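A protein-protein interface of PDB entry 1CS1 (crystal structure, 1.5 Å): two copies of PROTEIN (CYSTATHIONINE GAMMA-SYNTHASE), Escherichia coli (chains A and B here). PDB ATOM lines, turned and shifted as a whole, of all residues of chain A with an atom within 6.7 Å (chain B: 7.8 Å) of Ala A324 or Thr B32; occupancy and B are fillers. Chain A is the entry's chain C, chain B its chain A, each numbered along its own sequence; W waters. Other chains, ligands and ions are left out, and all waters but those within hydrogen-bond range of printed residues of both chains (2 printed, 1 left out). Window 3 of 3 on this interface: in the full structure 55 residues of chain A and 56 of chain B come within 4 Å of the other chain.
O of Ser A326 sits at hydrogen-bond distance from NH2 of Arg A361, 3.2 Å away. OG of Ser A204 sits at hydrogen-bond distance from OE2 of Glu A331 (2.7 Å). OG of Ser B30 is in hydrogen-bond range of O of Thr B32, at 2.8 Å. The backbone carbonyl oxygen (O) of Thr A322 is in hydrogen-bond range of the backbone NH (N) of Ile A334 (3.0 Å). The side-chain hydroxyl (OG1) of Thr B32 lies within hydrogen-bond range of the backbone carbonyl oxygen (O) of Asp B45, at 3.5 Å. The backbone NH (N) of His A336 is in hydrogen-bond range of the side-chain sulfur (SD) of Met A340 (3.5 Å).
The backbone carbonyl oxygen (O) of Leu B29 lies close to the backbone carbonyl oxygen (O) of Asp A205 (3.5 Å). N of Ser B31 sits at hydrogen-bond distance from O of Ser A204, 2.8 Å away. The side-chain hydroxyl of Thr B32 lies within hydrogen-bond range of the backbone carbonyl oxygen of Glu A325 (3.0 Å). The backbone carbonyl oxygen (O) of Leu A323 is in hydrogen-bond range of the backbone NH (N) of Phe B35 (2.9 Å).
Water W2 lies within hydrogen-bond range of the backbone NH of Glu A325 (2.7 Å), the backbone carbonyl oxygen of Tyr B33 (2.8 Å), the backbone carbonyl oxygen of Asp B45 (3.0 Å) and the side-chain hydroxyl of Thr B32 (3.4 Å). Water W1 lies within hydrogen-bond range of the side-chain hydroxyl (OG) of Ser A326 (2.8 Å) and the side-chain hydroxyl (OG) of Ser B31 (2.9 Å).
Of chain B, only Thr B32 (3.8 Å) and Tyr B33 (3.5 Å) come within 4 Å of Ala A324. Thr B32 touches two residues of chain A. Of the printed residues of chain A, Tyr B46 touches Ser A326 (3.5 Å). Of the printed residues of chain A, Ser B31 touches Ser A204. Of the printed residues of chain B, Thr A322 touches Asn B34 (3.5 Å). Of the printed residues of chain A, Ser B30 touches Ser A204 (3.2 Å). Of the printed residues of chain A, Leu B29 touches Ser A204 (3.9 Å) and Asp A205 (3.2 Å). His A336 touches none of the printed residues of chain B. Ser B47 touches none of the printed residues of chain A. The nearest residue of chain B that does not touch Ala A324 is Asn B34 (4.02 Å). The nearest residue of chain A that does not touch Thr B32 is Ser A326 (4.2 Å).
Of the 14 printed residues of chain B, 9 touch a printed residue of chain A. Printed residues of chain B that touch a printed residue of chain A: Leu B29, Ser B30, Ser B31, Thr B32, Tyr B33, Asn B34, Phe B35, Asp B45 and Tyr B46. Hydrophobic or aromatic side chains of chain B that line the printed part of chain A: Leu B29, Phe B35 and Tyr B46. Hydrophobic or aromatic side chains of chain A that line the printed part of chain B: Leu A323, Ala A324 and Met A340. Among the printed residues, no Asp or Glu carboxylate lies within 4 Å of a Lys or Arg side-chain nitrogen of the other chain.
No position is printed for both chains. Of the 13 pairs that touch across the chains among the printed residues, none has its exchanged pair printed and touching as well.
Among the printed residues, pairs that only touch across the chains: Ser A204 with Leu B29 (3.9 Å), Ser A204 with Ser B30 (3.2 Å), Thr A322 with Asn B34 (3.5 Å), Leu A323 with Asn B34 (3.4 Å), Ala A324 with Thr B32 (3.8 Å), Ala A324 with Tyr B33 (3.5 Å), Glu A325 with Asp B45 (3.4 Å), Ser A326 with Tyr B46 (3.5 Å) and Met A340 with Phe B35 (3.4 Å).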
ATOM      1  N   SER A 204       5.805 -31.173  14.821  1.00  0.00           N
ATOM      2  CA  SER A 204       5.797 -30.918  16.276  1.00  0.00           C
ATOM      3  C   SER A 204       4.861 -31.797  17.131  1.00  0.00           C
ATOM      4  O   SER A 204       4.340 -31.341  18.149  1.00  0.00           O
ATOM      5  CB  SER A 204       5.448 -29.445  16.534  1.00  0.00           C
ATOM      6  OG  SER A 204       6.020 -28.609  15.552  1.00  0.00           O
ATOM      7  N   ASP A 205       4.654 -33.049  16.734  1.00  0.00           N
ATOM      8  CA  ASP A 205       3.764 -33.923  17.485  1.00  0.00           C
ATOM      9  C   ASP A 205       4.361 -35.319  17.650  1.00  0.00           C
ATOM     10  O   ASP A 205       3.660 -36.280  17.947  1.00  0.00           O
ATOM     11  CB  ASP A 205       2.405 -34.005  16.781  1.00  0.00           C
ATOM     12  CG  ASP A 205       2.520 -34.459  15.325  1.00  0.00           C
ATOM     13  OD1 ASP A 205       1.487 -34.413  14.615  1.00  0.00           O
ATOM     14  OD2 ASP A 205       3.623 -34.861  14.891  1.00  0.00           O
ATOM     15  N   PHE A 321       5.041 -15.738  14.943  1.00  0.00           N
ATOM     16  CA  PHE A 321       6.218 -16.422  15.475  1.00  0.00           C
ATOM     17  C   PHE A 321       5.860 -16.723  16.917  1.00  0.00           C
ATOM     18  O   PHE A 321       5.568 -15.806  17.701  1.00  0.00           O
ATOM     19  CB  PHE A 321       7.466 -15.527  15.443  1.00  0.00           C
ATOM     20  CG  PHE A 321       8.012 -15.296  14.070  1.00  0.00           C
ATOM     21  CD1 PHE A 321       7.532 -14.251  13.286  1.00  0.00           C
ATOM     22  CD2 PHE A 321       8.961 -16.153  13.536  1.00  0.00           C
ATOM     23  CE1 PHE A 321       7.980 -14.068  11.993  1.00  0.00           C
ATOM     24  CE2 PHE A 321       9.423 -15.983  12.239  1.00  0.00           C
ATOM     25  CZ  PHE A 321       8.926 -14.935  11.462  1.00  0.00           C
ATOM     26  N   THR A 322       5.868 -18.006  17.259  1.00  0.00           N
ATOM     27  CA  THR A 322       5.525 -18.422  18.605  1.00  0.00           C
ATOM     28  C   THR A 322       6.784 -18.506  19.443  1.00  0.00           C
ATOM     29  O   THR A 322       7.767 -19.111  19.025  1.00  0.00           O
ATOM     30  CB  THR A 322       4.812 -19.821  18.599  1.00  0.00           C
ATOM     31  OG1 THR A 322       3.599 -19.743  17.829  1.00  0.00           O
ATOM     32  CG2 THR A 322       4.475 -20.270  20.031  1.00  0.00           C
ATOM     33  N   LEU A 323       6.762 -17.878  20.612  1.00  0.00           N
ATOM     34  CA  LEU A 323       7.902 -17.930  21.515  1.00  0.00           C
ATOM     35  C   LEU A 323       7.882 -19.314  22.173  1.00  0.00           C
ATOM     36  O   LEU A 323       7.058 -19.587  23.052  1.00  0.00           O
ATOM     37  CB  LEU A 323       7.783 -16.846  22.589  1.00  0.00           C
ATOM     38  CG  LEU A 323       8.967 -16.774  23.563  1.00  0.00           C
ATOM     39  CD1 LEU A 323      10.188 -16.262  22.819  1.00  0.00           C
ATOM     40  CD2 LEU A 323       8.645 -15.867  24.741  1.00  0.00           C
ATOM     41  N   ALA A 324       8.795 -20.180  21.750  1.00  0.00           N
ATOM     42  CA  ALA A 324       8.851 -21.529  22.279  1.00  0.00           C
ATOM     43  C   ALA A 324      10.168 -22.201  21.918  1.00  0.00           C
ATOM     44  O   ALA A 324      10.879 -21.737  21.027  1.00  0.00           O
ATOM     45  CB  ALA A 324       7.689 -22.335  21.704  1.00  0.00           C
ATOM     46  N   GLU A 325      10.480 -23.293  22.619  1.00  0.00           N
ATOM     47  CA  GLU A 325      11.690 -24.077  22.362  1.00  0.00           C
ATOM     48  C   GLU A 325      11.437 -24.958  21.142  1.00  0.00           C
ATOM     49  O   GLU A 325      10.311 -25.097  20.681  1.00  0.00           O
ATOM     50  CB  GLU A 325      12.021 -25.024  23.527  1.00  0.00           C
ATOM     51  CG  GLU A 325      11.849 -24.457  24.900  1.00  0.00           C
ATOM     52  CD  GLU A 325      13.135 -23.900  25.446  1.00  0.00           C
ATOM     53  OE1 GLU A 325      14.058 -23.682  24.637  1.00  0.00           O
ATOM     54  OE2 GLU A 325      13.223 -23.680  26.678  1.00  0.00           O
ATOM     55  N   SER A 326      12.499 -25.584  20.665  1.00  0.00           N
ATOM     56  CA  SER A 326      12.464 -26.480  19.524  1.00  0.00           C
ATOM     57  C   SER A 326      12.497 -25.760  18.183  1.00  0.00           C
ATOM     58  O   SER A 326      12.549 -24.529  18.121  1.00  0.00           O
ATOM     59  CB  SER A 326      11.260 -27.429  19.591  1.00  0.00           C
ATOM     60  OG  SER A 326      11.601 -28.665  18.982  1.00  0.00           O
ATOM     61  N   LEU A 327      12.480 -26.558  17.118  1.00  0.00           N
ATOM     62  CA  LEU A 327      12.553 -26.056  15.757  1.00  0.00           C
ATOM     63  C   LEU A 327      12.211 -27.213  14.817  1.00  0.00           C
ATOM     64  O   LEU A 327      12.011 -28.347  15.264  1.00  0.00           O
ATOM     65  CB  LEU A 327      13.989 -25.600  15.473  1.00  0.00           C
ATOM     66  CG  LEU A 327      15.037 -26.691  15.766  1.00  0.00           C
ATOM     67  CD1 LEU A 327      15.476 -27.394  14.490  1.00  0.00           C
ATOM     68  CD2 LEU A 327      16.239 -26.058  16.435  1.00  0.00           C
ATOM     69  N   GLU A 331       5.348 -24.662  11.532  1.00  0.00           N
ATOM     70  CA  GLU A 331       5.019 -23.354  12.080  1.00  0.00           C
ATOM     71  C   GLU A 331       6.293 -22.611  12.509  1.00  0.00           C
ATOM     72  O   GLU A 331       7.255 -23.214  12.995  1.00  0.00           O
ATOM     73  CB  GLU A 331       4.047 -23.504  13.260  1.00  0.00           C
ATOM     74  CG  GLU A 331       4.668 -23.991  14.585  1.00  0.00           C
ATOM     75  CD  GLU A 331       4.965 -25.488  14.599  1.00  0.00           C
ATOM     76  OE1 GLU A 331       4.571 -26.193  13.639  1.00  0.00           O
ATOM     77  OE2 GLU A 331       5.598 -25.959  15.576  1.00  0.00           O
ATOM     78  N   LEU A 333       8.794 -20.432  14.653  1.00  0.00           N
ATOM     79  CA  LEU A 333       9.065 -20.196  16.073  1.00  0.00           C
ATOM     80  C   LEU A 333      10.246 -19.247  16.279  1.00  0.00           C
ATOM     81  O   LEU A 333      11.092 -19.085  15.395  1.00  0.00           O
ATOM     82  CB  LEU A 333       9.380 -21.514  16.801  1.00  0.00           C
ATOM     83  CG  LEU A 333       8.402 -22.692  16.732  1.00  0.00           C
ATOM     84  CD1 LEU A 333       9.080 -23.940  17.318  1.00  0.00           C
ATOM     85  CD2 LEU A 333       7.113 -22.343  17.499  1.00  0.00           C
ATOM     86  N   ILE A 334      10.297 -18.632  17.455  1.00  0.00           N
ATOM     87  CA  ILE A 334      11.381 -17.731  17.794  1.00  0.00           C
ATOM     88  C   ILE A 334      11.752 -17.949  19.256  1.00  0.00           C
ATOM     89  O   ILE A 334      10.881 -18.208  20.100  1.00  0.00           O
ATOM     90  CB  ILE A 334      10.994 -16.254  17.576  1.00  0.00           C
ATOM     91  CG1 ILE A 334      12.241 -15.375  17.728  1.00  0.00           C
ATOM     92  CG2 ILE A 334       9.924 -15.831  18.563  1.00  0.00           C
ATOM     93  CD1 ILE A 334      11.946 -13.903  17.789  1.00  0.00           C
ATOM     94  N   SER A 335      13.046 -17.866  19.550  1.00  0.00           N
ATOM     95  CA  SER A 335      13.518 -18.054  20.914  1.00  0.00           C
ATOM     96  C   SER A 335      14.637 -17.091  21.274  1.00  0.00           C
ATOM     97  O   SER A 335      15.373 -16.616  20.409  1.00  0.00           O
ATOM     98  CB  SER A 335      14.007 -19.491  21.119  1.00  0.00           C
ATOM     99  OG  SER A 335      14.830 -19.905  20.044  1.00  0.00           O
ATOM    100  N   HIS A 336      14.740 -16.825  22.571  1.00  0.00           N
ATOM    101  CA  HIS A 336      15.740 -15.938  23.162  1.00  0.00           C
ATOM    102  C   HIS A 336      16.730 -16.837  23.920  1.00  0.00           C
ATOM    103  O   HIS A 336      16.490 -17.204  25.062  1.00  0.00           O
ATOM    104  CB  HIS A 336      15.039 -14.981  24.127  1.00  0.00           C
ATOM    105  CG  HIS A 336      15.961 -14.040  24.830  1.00  0.00           C
ATOM    106  ND1 HIS A 336      16.039 -13.966  26.204  1.00  0.00           N
ATOM    107  CD2 HIS A 336      16.827 -13.114  24.356  1.00  0.00           C
ATOM    108  CE1 HIS A 336      16.914 -13.041  26.546  1.00  0.00           C
ATOM    109  NE2 HIS A 336      17.406 -12.507  25.443  1.00  0.00           N
ATOM    110  N   MET A 340      16.196 -18.866  27.118  1.00  0.00           N
ATOM    111  CA  MET A 340      15.741 -20.218  26.854  1.00  0.00           C
ATOM    112  C   MET A 340      16.898 -21.189  26.631  1.00  0.00           C
ATOM    113  O   MET A 340      17.414 -21.783  27.581  1.00  0.00           O
ATOM    114  CB  MET A 340      14.788 -20.186  25.656  1.00  0.00           C
ATOM    115  CG  MET A 340      13.665 -19.179  25.877  1.00  0.00           C
ATOM    116  SD  MET A 340      12.578 -18.812  24.482  1.00  0.00           S
ATOM    117  CE  MET A 340      11.574 -17.645  25.240  1.00  0.00           C
ATOM    118  N   ARG A 361      16.675 -16.375  17.928  1.00  0.00           N
ATOM    119  CA  ARG A 361      16.776 -17.388  16.887  1.00  0.00           C
ATOM    120  C   ARG A 361      15.408 -17.663  16.270  1.00  0.00           C
ATOM    121  O   ARG A 361      14.402 -17.763  16.968  1.00  0.00           O
ATOM    122  CB  ARG A 361      17.339 -18.693  17.458  1.00  0.00           C
ATOM    123  CG  ARG A 361      17.576 -19.772  16.416  1.00  0.00           C
ATOM    124  CD  ARG A 361      17.837 -21.114  17.091  1.00  0.00           C
ATOM    125  NE  ARG A 361      16.607 -21.694  17.625  1.00  0.00           N
ATOM    126  CZ  ARG A 361      16.559 -22.716  18.476  1.00  0.00           C
ATOM    127  NH1 ARG A 361      17.673 -23.289  18.904  1.00  0.00           N
ATOM    128  NH2 ARG A 361      15.388 -23.170  18.897  1.00  0.00           N
ATOM    129  N   LEU B  29       0.101 -34.402  22.065  1.00  0.00           N
ATOM    130  CA  LEU B  29       1.217 -34.882  21.256  1.00  0.00           C
ATOM    131  C   LEU B  29       2.286 -33.814  21.025  1.00  0.00           C
ATOM    132  O   LEU B  29       3.429 -34.141  20.681  1.00  0.00           O
ATOM    133  CB  LEU B  29       0.711 -35.384  19.893  1.00  0.00           C
ATOM    134  CG  LEU B  29      -0.236 -36.590  19.877  1.00  0.00           C
ATOM    135  CD1 LEU B  29      -0.619 -36.901  18.425  1.00  0.00           C
ATOM    136  CD2 LEU B  29       0.432 -37.811  20.561  1.00  0.00           C
ATOM    137  N   SER B  30       1.907 -32.549  21.212  1.00  0.00           N
ATOM    138  CA  SER B  30       2.817 -31.417  20.996  1.00  0.00           C
ATOM    139  C   SER B  30       4.210 -31.584  21.630  1.00  0.00           C
ATOM    140  O   SER B  30       4.348 -31.843  22.828  1.00  0.00           O
ATOM    141  CB  SER B  30       2.168 -30.122  21.492  1.00  0.00           C
ATOM    142  OG  SER B  30       2.831 -28.996  20.948  1.00  0.00           O
ATOM    143  N   SER B  31       5.239 -31.438  20.801  1.00  0.00           N
ATOM    144  CA  SER B  31       6.620 -31.567  21.243  1.00  0.00           C
ATOM    145  C   SER B  31       7.062 -30.343  22.040  1.00  0.00           C
ATOM    146  O   SER B  31       8.031 -30.404  22.808  1.00  0.00           O
ATOM    147  CB  SER B  31       7.536 -31.728  20.033  1.00  0.00           C
ATOM    148  OG  SER B  31       7.415 -30.621  19.146  1.00  0.00           O
ATOM    149  N   THR B  32       6.350 -29.232  21.857  1.00  0.00           N
ATOM    150  CA  THR B  32       6.693 -28.008  22.560  1.00  0.00           C
ATOM    151  C   THR B  32       5.504 -27.177  23.037  1.00  0.00           C
ATOM    152  O   THR B  32       4.358 -27.407  22.645  1.00  0.00           O
ATOM    153  CB  THR B  32       7.621 -27.140  21.701  1.00  0.00           C
ATOM    154  OG1 THR B  32       8.044 -26.010  22.479  1.00  0.00           O
ATOM    155  CG2 THR B  32       6.911 -26.693  20.402  1.00  0.00           C
ATOM    156  N   TYR B  33       5.791 -26.202  23.893  1.00  0.00           N
ATOM    157  CA  TYR B  33       4.759 -25.350  24.486  1.00  0.00           C
ATOM    158  C   TYR B  33       5.149 -23.880  24.436  1.00  0.00           C
ATOM    159  O   TYR B  33       6.294 -23.532  24.707  1.00  0.00           O
ATOM    160  CB  TYR B  33       4.539 -25.761  25.952  1.00  0.00           C
ATOM    161  CG  TYR B  33       4.559 -27.262  26.142  1.00  0.00           C
ATOM    162  CD1 TYR B  33       5.772 -27.967  26.199  1.00  0.00           C
ATOM    163  CD2 TYR B  33       3.365 -27.991  26.169  1.00  0.00           C
ATOM    164  CE1 TYR B  33       5.789 -29.369  26.263  1.00  0.00           C
ATOM    165  CE2 TYR B  33       3.371 -29.377  26.231  1.00  0.00           C
ATOM    166  CZ  TYR B  33       4.580 -30.062  26.271  1.00  0.00           C
ATOM    167  OH  TYR B  33       4.572 -31.437  26.269  1.00  0.00           O
ATOM    168  N   ASN B  34       4.199 -23.013  24.110  1.00  0.00           N
ATOM    169  CA  ASN B  34       4.511 -21.597  24.057  1.00  0.00           C
ATOM    170  C   ASN B  34       4.701 -21.031  25.455  1.00  0.00           C
ATOM    171  O   ASN B  34       4.131 -21.536  26.436  1.00  0.00           O
ATOM    172  CB  ASN B  34       3.420 -20.823  23.314  1.00  0.00           C
ATOM    173  CG  ASN B  34       2.100 -20.829  24.041  1.00  0.00           C
ATOM    174  OD1 ASN B  34       1.971 -20.298  25.152  1.00  0.00           O
ATOM    175  ND2 ASN B  34       1.094 -21.429  23.411  1.00  0.00           N
ATOM    176  N   PHE B  35       5.533 -19.996  25.538  1.00  0.00           N
ATOM    177  CA  PHE B  35       5.818 -19.322  26.802  1.00  0.00           C
ATOM    178  C   PHE B  35       4.668 -18.375  27.106  1.00  0.00           C
ATOM    179  O   PHE B  35       4.067 -17.812  26.191  1.00  0.00           O
ATOM    180  CB  PHE B  35       7.100 -18.485  26.692  1.00  0.00           C
ATOM    181  CG  PHE B  35       8.343 -19.215  27.075  1.00  0.00           C
ATOM    182  CD1 PHE B  35       8.501 -20.560  26.770  1.00  0.00           C
ATOM    183  CD2 PHE B  35       9.377 -18.542  27.720  1.00  0.00           C
ATOM    184  CE1 PHE B  35       9.672 -21.225  27.096  1.00  0.00           C
ATOM    185  CE2 PHE B  35      10.553 -19.199  28.050  1.00  0.00           C
ATOM    186  CZ  PHE B  35      10.703 -20.546  27.738  1.00  0.00           C
ATOM    187  N   HIS B  44       5.362 -26.744  31.457  1.00  0.00           N
ATOM    188  CA  HIS B  44       6.089 -27.559  30.488  1.00  0.00           C
ATOM    189  C   HIS B  44       6.692 -26.650  29.411  1.00  0.00           C
ATOM    190  O   HIS B  44       6.098 -25.623  29.053  1.00  0.00           O
ATOM    191  CB  HIS B  44       5.139 -28.573  29.809  1.00  0.00           C
ATOM    192  CG  HIS B  44       4.287 -29.365  30.761  1.00  0.00           C
ATOM    193  ND1 HIS B  44       3.076 -28.910  31.238  1.00  0.00           N
ATOM    194  CD2 HIS B  44       4.460 -30.598  31.296  1.00  0.00           C
ATOM    195  CE1 HIS B  44       2.538 -29.825  32.024  1.00  0.00           C
ATOM    196  NE2 HIS B  44       3.358 -30.859  32.075  1.00  0.00           N
ATOM    197  N   ASP B  45       7.865 -27.015  28.898  1.00  0.00           N
ATOM    198  CA  ASP B  45       8.485 -26.241  27.819  1.00  0.00           C
ATOM    199  C   ASP B  45       9.021 -27.159  26.715  1.00  0.00           C
ATOM    200  O   ASP B  45       9.354 -26.716  25.616  1.00  0.00           O
ATOM    201  CB  ASP B  45       9.602 -25.329  28.347  1.00  0.00           C
ATOM    202  CG  ASP B  45      10.480 -26.004  29.373  1.00  0.00           C
ATOM    203  OD1 ASP B  45      11.411 -26.740  28.979  1.00  0.00           O
ATOM    204  OD2 ASP B  45      10.243 -25.790  30.581  1.00  0.00           O
ATOM    205  N   TYR B  46       9.099 -28.449  27.002  1.00  0.00           N
ATOM    206  CA  TYR B  46       9.563 -29.394  26.001  1.00  0.00           C
ATOM    207  C   TYR B  46       9.130 -30.806  26.407  1.00  0.00           C
ATOM    208  O   TYR B  46       9.551 -31.336  27.444  1.00  0.00           O
ATOM    209  CB  TYR B  46      11.089 -29.302  25.849  1.00  0.00           C
ATOM    210  CG  TYR B  46      11.626 -29.972  24.593  1.00  0.00           C
ATOM    211  CD1 TYR B  46      12.432 -31.115  24.678  1.00  0.00           C
ATOM    212  CD2 TYR B  46      11.317 -29.476  23.321  1.00  0.00           C
ATOM    213  CE1 TYR B  46      12.919 -31.755  23.523  1.00  0.00           C
ATOM    214  CE2 TYR B  46      11.800 -30.109  22.160  1.00  0.00           C
ATOM    215  CZ  TYR B  46      12.600 -31.247  22.273  1.00  0.00           C
ATOM    216  OH  TYR B  46      13.077 -31.882  21.146  1.00  0.00           O
ATOM    217  N   SER B  47       8.282 -31.400  25.575  1.00  0.00           N
ATOM    218  CA  SER B  47       7.732 -32.729  25.823  1.00  0.00           C
ATOM    219  C   SER B  47       8.692 -33.828  26.310  1.00  0.00           C
ATOM    220  O   SER B  47       8.313 -34.669  27.127  1.00  0.00           O
ATOM    221  CB  SER B  47       7.001 -33.216  24.563  1.00  0.00           C
ATOM    222  OG  SER B  47       6.344 -34.456  24.790  1.00  0.00           O
ATOM    223  N   ARG B  48       9.924 -33.836  25.808  1.00  0.00           N
ATOM    224  CA  ARG B  48      10.875 -34.871  26.212  1.00  0.00           C
ATOM    225  C   ARG B  48      11.138 -34.780  27.701  1.00  0.00           C
ATOM    226  O   ARG B  48      11.295 -35.797  28.385  1.00  0.00           O
ATOM    227  CB  ARG B  48      12.195 -34.728  25.446  1.00  0.00           C
ATOM    228  CG  ARG B  48      13.037 -35.974  25.499  1.00  0.00           C
ATOM    229  CD  ARG B  48      14.480 -35.653  25.756  1.00  0.00           C
ATOM    230  NE  ARG B  48      14.978 -34.693  24.783  1.00  0.00           N
ATOM    231  CZ  ARG B  48      15.543 -33.535  25.108  1.00  0.00           C
ATOM    232  NH1 ARG B  48      15.677 -33.202  26.389  1.00  0.00           N
ATOM    233  NH2 ARG B  48      15.984 -32.713  24.156  1.00  0.00           N
ATOM    234  N   GLY B  50       9.037 -32.871  29.964  1.00  0.00           N
ATOM    235  CA  GLY B  50       7.769 -32.923  30.676  1.00  0.00           C
ATOM    236  C   GLY B  50       6.628 -32.798  29.681  1.00  0.00           C
ATOM    237  O   GLY B  50       6.664 -31.942  28.803  1.00  0.00           O
ATOM    238  N   ASN B  51       5.620 -33.650  29.821  1.00  0.00           N
ATOM    239  CA  ASN B  51       4.453 -33.686  28.932  1.00  0.00           C
ATOM    240  C   ASN B  51       3.206 -33.828  29.828  1.00  0.00           C
ATOM    241  O   ASN B  51       3.215 -34.610  30.768  1.00  0.00           O
ATOM    242  CB  ASN B  51       4.615 -34.884  27.987  1.00  0.00           C
ATOM    243  CG  ASN B  51       3.400 -35.135  27.130  1.00  0.00           C
ATOM    244  OD1 ASN B  51       2.394 -35.646  27.596  1.00  0.00           O
ATOM    245  ND2 ASN B  51       3.502 -34.789  25.860  1.00  0.00           N
HETATM  246  O   HOH W   1       9.802 -30.205  17.519  1.00  0.00           O
HETATM  247  O   HOH W   2       9.047 -23.781  24.878  1.00  0.00           O
